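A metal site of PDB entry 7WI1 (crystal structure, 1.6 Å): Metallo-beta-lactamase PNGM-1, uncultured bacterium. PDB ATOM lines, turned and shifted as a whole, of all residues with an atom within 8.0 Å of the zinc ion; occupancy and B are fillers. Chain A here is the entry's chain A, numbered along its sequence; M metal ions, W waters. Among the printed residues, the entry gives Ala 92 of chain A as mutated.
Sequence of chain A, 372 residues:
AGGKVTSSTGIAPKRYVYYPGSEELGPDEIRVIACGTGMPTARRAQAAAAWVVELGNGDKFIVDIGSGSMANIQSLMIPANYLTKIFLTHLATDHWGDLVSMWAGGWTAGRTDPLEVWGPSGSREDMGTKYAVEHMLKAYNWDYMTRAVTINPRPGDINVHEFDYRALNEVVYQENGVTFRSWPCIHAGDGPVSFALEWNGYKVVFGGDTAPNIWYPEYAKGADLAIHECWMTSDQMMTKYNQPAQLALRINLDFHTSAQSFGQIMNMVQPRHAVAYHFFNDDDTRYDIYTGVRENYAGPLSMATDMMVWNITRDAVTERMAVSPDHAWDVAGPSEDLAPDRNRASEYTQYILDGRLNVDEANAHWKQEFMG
The zinc ion is bound by water W1, at 2.0 Å.
The zinc ion is bound by NE2 of His 278 (2.1 Å).
NE2 of His 95 is bound to the zinc ion (2.1 Å).
OD2 of Asp 209 binds the zinc ion (2.1 Å).
The side-chain carboxylate (OD2) of Asp 94 is bound to the zinc ion (2.3 Å).
Within 4 Å of the zinc ion: Asp 94, His 95, Asp 209 and His 278.
Along chain A the residues within 4 Å of the zinc ion span positions 94 to 278.
Water W1 lies within hydrogen-bond range of OD1 of Asp 94 (2.6 Å) and NE2 of His 90 (3.5 Å).
The side-chain carboxylate (OD2) of Asp 209 sits close to a ring nitrogen (NE2) of His 187 (3.2 Å).
The side-chain carboxylate (OD2) of Asp 209 sits close to a ring nitrogen (NE2) of His 90 (3.2 Å).
OD2 of Asp 64 is in hydrogen-bond range of ND1 of His 95, at 2.6 Å.
N of Ala 49 sits at hydrogen-bond distance from O of Asp 94 (3.3 Å).
A ring nitrogen (ND1) of His 278 sits at hydrogen-bond distance from the backbone carbonyl oxygen (O) of Gly 38, at 3.3 Å.
The side-chain hydroxyl of Tyr 277 lies within hydrogen-bond range of the side-chain carboxylate of Asp 209.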
ATOM      1  N   GLY A  38     -20.026  33.330 -23.929  1.00  0.00           N
ATOM      2  CA  GLY A  38     -20.579  32.960 -25.250  1.00  0.00           C
ATOM      3  C   GLY A  38     -21.650  31.888 -25.200  1.00  0.00           C
ATOM      4  O   GLY A  38     -22.566  31.980 -24.356  1.00  0.00           O
ATOM      5  N   MET A  39     -21.541  30.883 -26.074  1.00  0.00           N
ATOM      6  CA  MET A  39     -22.622  29.922 -26.428  1.00  0.00           C
ATOM      7  C   MET A  39     -22.000  28.547 -26.638  1.00  0.00           C
ATOM      8  O   MET A  39     -20.802  28.376 -26.481  1.00  0.00           O
ATOM      9  CB  MET A  39     -23.269  30.319 -27.754  1.00  0.00           C
ATOM     10  CG  MET A  39     -23.822  31.704 -27.787  1.00  0.00           C
ATOM     11  SD  MET A  39     -25.592  31.679 -28.022  1.00  0.00           S
ATOM     12  CE  MET A  39     -25.706  32.970 -29.251  1.00  0.00           C
ATOM     13  N   PRO A  40     -22.812  27.495 -26.864  1.00  0.00           N
ATOM     14  CA  PRO A  40     -22.263  26.167 -27.152  1.00  0.00           C
ATOM     15  C   PRO A  40     -21.479  26.054 -28.480  1.00  0.00           C
ATOM     16  O   PRO A  40     -20.665  25.159 -28.574  1.00  0.00           O
ATOM     17  CB  PRO A  40     -23.529  25.299 -27.207  1.00  0.00           C
ATOM     18  CG  PRO A  40     -24.557  26.081 -26.448  1.00  0.00           C
ATOM     19  CD  PRO A  40     -24.274  27.515 -26.823  1.00  0.00           C
ATOM     20  N   ALA A  48     -17.102  29.845 -23.634  1.00  0.00           N
ATOM     21  CA  ALA A  48     -18.383  29.537 -23.004  1.00  0.00           C
ATOM     22  C   ALA A  48     -18.335  30.086 -21.552  1.00  0.00           C
ATOM     23  O   ALA A  48     -17.236  30.252 -20.959  1.00  0.00           O
ATOM     24  CB  ALA A  48     -18.641  28.058 -23.084  1.00  0.00           C
ATOM     25  N   ALA A  49     -19.519  30.290 -20.999  1.00  0.00           N
ATOM     26  CA  ALA A  49     -19.810  30.826 -19.632  1.00  0.00           C
ATOM     27  C   ALA A  49     -18.765  30.441 -18.568  1.00  0.00           C
ATOM     28  O   ALA A  49     -18.571  29.248 -18.256  1.00  0.00           O
ATOM     29  CB  ALA A  49     -21.199  30.332 -19.205  1.00  0.00           C
ATOM     30  N   ASP A  64     -19.215  28.635 -12.912  1.00  0.00           N
ATOM     31  CA  ASP A  64     -19.268  28.067 -14.288  1.00  0.00           C
ATOM     32  C   ASP A  64     -17.867  28.079 -14.876  1.00  0.00           C
ATOM     33  O   ASP A  64     -17.035  28.872 -14.517  1.00  0.00           O
ATOM     34  CB  ASP A  64     -20.307  28.715 -15.211  1.00  0.00           C
ATOM     35  CG  ASP A  64     -21.752  28.341 -14.913  1.00  0.00           C
ATOM     36  OD1 ASP A  64     -21.879  27.390 -14.082  1.00  0.00           O
ATOM     37  OD2 ASP A  64     -22.731  28.971 -15.511  1.00  0.00           O
ATOM     38  N   THR A  89     -23.884  26.303 -12.389  1.00  0.00           N
ATOM     39  CA  THR A  89     -25.318  26.638 -12.561  1.00  0.00           C
ATOM     40  C   THR A  89     -26.069  25.461 -13.116  1.00  0.00           C
ATOM     41  O   THR A  89     -27.273  25.263 -12.762  1.00  0.00           O
ATOM     42  CB  THR A  89     -25.547  27.913 -13.361  1.00  0.00           C
ATOM     43  OG1 THR A  89     -25.054  27.762 -14.690  1.00  0.00           O
ATOM     44  CG2 THR A  89     -24.936  29.132 -12.703  1.00  0.00           C
ATOM     45  N   HIS A  90     -25.474  24.725 -14.062  1.00  0.00           N
ATOM     46  CA  HIS A  90     -26.106  23.580 -14.746  1.00  0.00           C
ATOM     47  C   HIS A  90     -25.035  22.860 -15.562  1.00  0.00           C
ATOM     48  O   HIS A  90     -23.863  23.299 -15.521  1.00  0.00           O
ATOM     49  CB  HIS A  90     -27.273  23.945 -15.664  1.00  0.00           C
ATOM     50  CG  HIS A  90     -26.989  24.808 -16.848  1.00  0.00           C
ATOM     51  ND1 HIS A  90     -26.459  26.098 -16.740  1.00  0.00           N
ATOM     52  CD2 HIS A  90     -27.313  24.660 -18.138  1.00  0.00           C
ATOM     53  CE1 HIS A  90     -26.484  26.685 -17.929  1.00  0.00           C
ATOM     54  NE2 HIS A  90     -26.977  25.844 -18.774  1.00  0.00           N
ATOM     55  N   ALA A  92     -24.760  21.818 -18.658  1.00  0.00           N
ATOM     56  CA  ALA A  92     -24.445  21.988 -20.099  1.00  0.00           C
ATOM     57  C   ALA A  92     -22.952  22.129 -20.341  1.00  0.00           C
ATOM     58  O   ALA A  92     -22.212  22.598 -19.505  1.00  0.00           O
ATOM     59  CB  ALA A  92     -25.173  23.143 -20.642  1.00  0.00           C
ATOM     60  N   THR A  93     -22.481  21.645 -21.513  1.00  0.00           N
ATOM     61  CA  THR A  93     -21.043  21.651 -21.872  1.00  0.00           C
ATOM     62  C   THR A  93     -20.534  23.095 -21.818  1.00  0.00           C
ATOM     63  O   THR A  93     -19.392  23.314 -21.451  1.00  0.00           O
ATOM     64  CB  THR A  93     -20.819  21.063 -23.280  1.00  0.00           C
ATOM     65  OG1 THR A  93     -21.376  21.894 -24.307  1.00  0.00           O
ATOM     66  CG2 THR A  93     -21.358  19.660 -23.338  1.00  0.00           C
ATOM     67  N   ASP A  94     -21.353  24.034 -22.150  1.00  0.00           N
ATOM     68  CA  ASP A  94     -20.955  25.471 -22.173  1.00  0.00           C
ATOM     69  C   ASP A  94     -20.939  26.068 -20.751  1.00  0.00           C
ATOM     70  O   ASP A  94     -20.660  27.262 -20.610  1.00  0.00           O
ATOM     71  CB  ASP A  94     -21.784  26.277 -23.178  1.00  0.00           C
ATOM     72  CG  ASP A  94     -23.243  26.433 -22.826  1.00  0.00           C
ATOM     73  OD1 ASP A  94     -23.918  25.386 -22.571  1.00  0.00           O
ATOM     74  OD2 ASP A  94     -23.739  27.618 -22.754  1.00  0.00           O
ATOM     75  N   HIS A  95     -21.201  25.275 -19.707  1.00  0.00           N
ATOM     76  CA  HIS A  95     -21.026  25.705 -18.278  1.00  0.00           C
ATOM     77  C   HIS A  95     -20.058  24.846 -17.480  1.00  0.00           C
ATOM     78  O   HIS A  95     -19.650  25.291 -16.411  1.00  0.00           O
ATOM     79  CB  HIS A  95     -22.400  25.811 -17.640  1.00  0.00           C
ATOM     80  CG  HIS A  95     -23.246  26.824 -18.346  1.00  0.00           C
ATOM     81  ND1 HIS A  95     -23.399  28.148 -17.859  1.00  0.00           N
ATOM     82  CD2 HIS A  95     -23.840  26.816 -19.558  1.00  0.00           C
ATOM     83  CE1 HIS A  95     -24.141  28.819 -18.712  1.00  0.00           C
ATOM     84  NE2 HIS A  95     -24.355  28.040 -19.803  1.00  0.00           N
ATOM     85  N   HIS A 187     -34.897  26.110 -18.016  1.00  0.00           N
ATOM     86  CA  HIS A 187     -33.889  26.003 -19.111  1.00  0.00           C
ATOM     87  C   HIS A 187     -33.721  24.520 -19.502  1.00  0.00           C
ATOM     88  O   HIS A 187     -32.948  23.814 -18.776  1.00  0.00           O
ATOM     89  CB  HIS A 187     -32.588  26.590 -18.603  1.00  0.00           C
ATOM     90  CG  HIS A 187     -31.487  26.555 -19.605  1.00  0.00           C
ATOM     91  ND1 HIS A 187     -31.578  27.274 -20.753  1.00  0.00           N
ATOM     92  CD2 HIS A 187     -30.262  25.975 -19.609  1.00  0.00           C
ATOM     93  CE1 HIS A 187     -30.469  27.138 -21.443  1.00  0.00           C
ATOM     94  NE2 HIS A 187     -29.662  26.355 -20.794  1.00  0.00           N
ATOM     95  N   GLY A 208     -26.863  32.309 -14.447  1.00  0.00           N
ATOM     96  CA  GLY A 208     -26.779  31.053 -15.225  1.00  0.00           C
ATOM     97  C   GLY A 208     -27.647  31.226 -16.459  1.00  0.00           C
ATOM     98  O   GLY A 208     -27.556  32.302 -17.057  1.00  0.00           O
ATOM     99  N   ASP A 209     -28.420  30.209 -16.834  1.00  0.00           N
ATOM    100  CA  ASP A 209     -29.301  30.227 -18.027  1.00  0.00           C
ATOM    101  C   ASP A 209     -30.739  30.065 -17.606  1.00  0.00           C
ATOM    102  O   ASP A 209     -30.998  29.191 -16.760  1.00  0.00           O
ATOM    103  CB  ASP A 209     -28.984  29.105 -19.018  1.00  0.00           C
ATOM    104  CG  ASP A 209     -27.634  29.287 -19.681  1.00  0.00           C
ATOM    105  OD1 ASP A 209     -26.866  30.143 -19.202  1.00  0.00           O
ATOM    106  OD2 ASP A 209     -27.343  28.479 -20.575  1.00  0.00           O
ATOM    107  N   THR A 210     -31.639  30.807 -18.217  1.00  0.00           N
ATOM    108  CA  THR A 210     -33.088  30.657 -17.886  1.00  0.00           C
ATOM    109  C   THR A 210     -33.922  31.421 -18.900  1.00  0.00           C
ATOM    110  O   THR A 210     -33.497  32.497 -19.364  1.00  0.00           O
ATOM    111  CB  THR A 210     -33.400  31.127 -16.444  1.00  0.00           C
ATOM    112  OG1 THR A 210     -34.734  30.671 -16.087  1.00  0.00           O
ATOM    113  CG2 THR A 210     -33.269  32.625 -16.203  1.00  0.00           C
ATOM    114  N   GLU A 229     -28.853  35.945 -18.418  1.00  0.00           N
ATOM    115  CA  GLU A 229     -28.811  35.629 -19.867  1.00  0.00           C
ATOM    116  C   GLU A 229     -29.634  36.678 -20.568  1.00  0.00           C
ATOM    117  O   GLU A 229     -30.651  37.175 -19.993  1.00  0.00           O
ATOM    118  CB  GLU A 229     -29.291  34.198 -20.154  1.00  0.00           C
ATOM    119  CG  GLU A 229     -30.660  34.128 -20.765  1.00  0.00           C
ATOM    120  CD  GLU A 229     -31.071  32.765 -21.284  1.00  0.00           C
ATOM    121  OE1 GLU A 229     -30.572  31.727 -20.752  1.00  0.00           O
ATOM    122  OE2 GLU A 229     -31.901  32.733 -22.202  1.00  0.00           O
ATOM    123  N   TRP A 231     -30.575  37.355 -24.803  1.00  0.00           N
ATOM    124  CA  TRP A 231     -30.455  36.613 -26.073  1.00  0.00           C
ATOM    125  C   TRP A 231     -30.300  37.539 -27.260  1.00  0.00           C
ATOM    126  O   TRP A 231     -30.816  38.696 -27.250  1.00  0.00           O
ATOM    127  CB  TRP A 231     -31.644  35.689 -26.321  1.00  0.00           C
ATOM    128  CG  TRP A 231     -31.255  34.446 -27.026  1.00  0.00           C
ATOM    129  CD1 TRP A 231     -31.566  34.038 -28.292  1.00  0.00           C
ATOM    130  CD2 TRP A 231     -30.463  33.400 -26.452  1.00  0.00           C
ATOM    131  NE1 TRP A 231     -30.972  32.825 -28.546  1.00  0.00           N
ATOM    132  CE2 TRP A 231     -30.289  32.422 -27.443  1.00  0.00           C
ATOM    133  CE3 TRP A 231     -29.812  33.255 -25.226  1.00  0.00           C
ATOM    134  CZ2 TRP A 231     -29.515  31.284 -27.227  1.00  0.00           C
ATOM    135  CZ3 TRP A 231     -29.082  32.108 -25.001  1.00  0.00           C
ATOM    136  CH2 TRP A 231     -28.923  31.152 -26.000  1.00  0.00           C
ATOM    137  N   HIS A 256     -35.676  31.315 -24.342  1.00  0.00           N
ATOM    138  CA  HIS A 256     -34.642  32.218 -23.771  1.00  0.00           C
ATOM    139  C   HIS A 256     -35.234  33.544 -23.290  1.00  0.00           C
ATOM    140  O   HIS A 256     -36.388  33.874 -23.629  1.00  0.00           O
ATOM    141  CB  HIS A 256     -33.564  32.461 -24.829  1.00  0.00           C
ATOM    142  CG  HIS A 256     -32.828  31.190 -25.139  1.00  0.00           C
ATOM    143  ND1 HIS A 256     -31.942  30.612 -24.252  1.00  0.00           N
ATOM    144  CD2 HIS A 256     -32.902  30.371 -26.209  1.00  0.00           C
ATOM    145  CE1 HIS A 256     -31.468  29.499 -24.785  1.00  0.00           C
ATOM    146  NE2 HIS A 256     -32.040  29.327 -25.976  1.00  0.00           N
ATOM    147  N   TYR A 277     -25.272  38.763 -20.640  1.00  0.00           N
ATOM    148  CA  TYR A 277     -24.291  37.827 -21.245  1.00  0.00           C
ATOM    149  C   TYR A 277     -25.025  36.752 -22.035  1.00  0.00           C
ATOM    150  O   TYR A 277     -26.269  36.667 -22.074  1.00  0.00           O
ATOM    151  CB  TYR A 277     -23.333  37.276 -20.178  1.00  0.00           C
ATOM    152  CG  TYR A 277     -23.743  35.979 -19.566  1.00  0.00           C
ATOM    153  CD1 TYR A 277     -24.930  35.873 -18.853  1.00  0.00           C
ATOM    154  CD2 TYR A 277     -23.004  34.827 -19.778  1.00  0.00           C
ATOM    155  CE1 TYR A 277     -25.312  34.660 -18.306  1.00  0.00           C
ATOM    156  CE2 TYR A 277     -23.392  33.604 -19.247  1.00  0.00           C
ATOM    157  CZ  TYR A 277     -24.555  33.524 -18.509  1.00  0.00           C
ATOM    158  OH  TYR A 277     -24.962  32.299 -18.020  1.00  0.00           O
ATOM    159  N   HIS A 278     -24.205  35.887 -22.660  1.00  0.00           N
ATOM    160  CA  HIS A 278     -24.624  34.625 -23.302  1.00  0.00           C
ATOM    161  C   HIS A 278     -25.136  34.954 -24.699  1.00  0.00           C
ATOM    162  O   HIS A 278     -25.907  34.190 -25.261  1.00  0.00           O
ATOM    163  CB  HIS A 278     -25.668  33.863 -22.450  1.00  0.00           C
ATOM    164  CG  HIS A 278     -25.617  32.381 -22.597  1.00  0.00           C
ATOM    165  ND1 HIS A 278     -25.780  31.740 -23.847  1.00  0.00           N
ATOM    166  CD2 HIS A 278     -25.414  31.417 -21.686  1.00  0.00           C
ATOM    167  CE1 HIS A 278     -25.736  30.435 -23.630  1.00  0.00           C
ATOM    168  NE2 HIS A 278     -25.392  30.241 -22.355  1.00  0.00           N
HETATM  169 ZN    ZN M   1     -25.468  28.362 -21.512  1.00  0.00          ZN
HETATM  170  O   HOH W   1     -26.195  26.538 -22.089  1.00  0.00           O
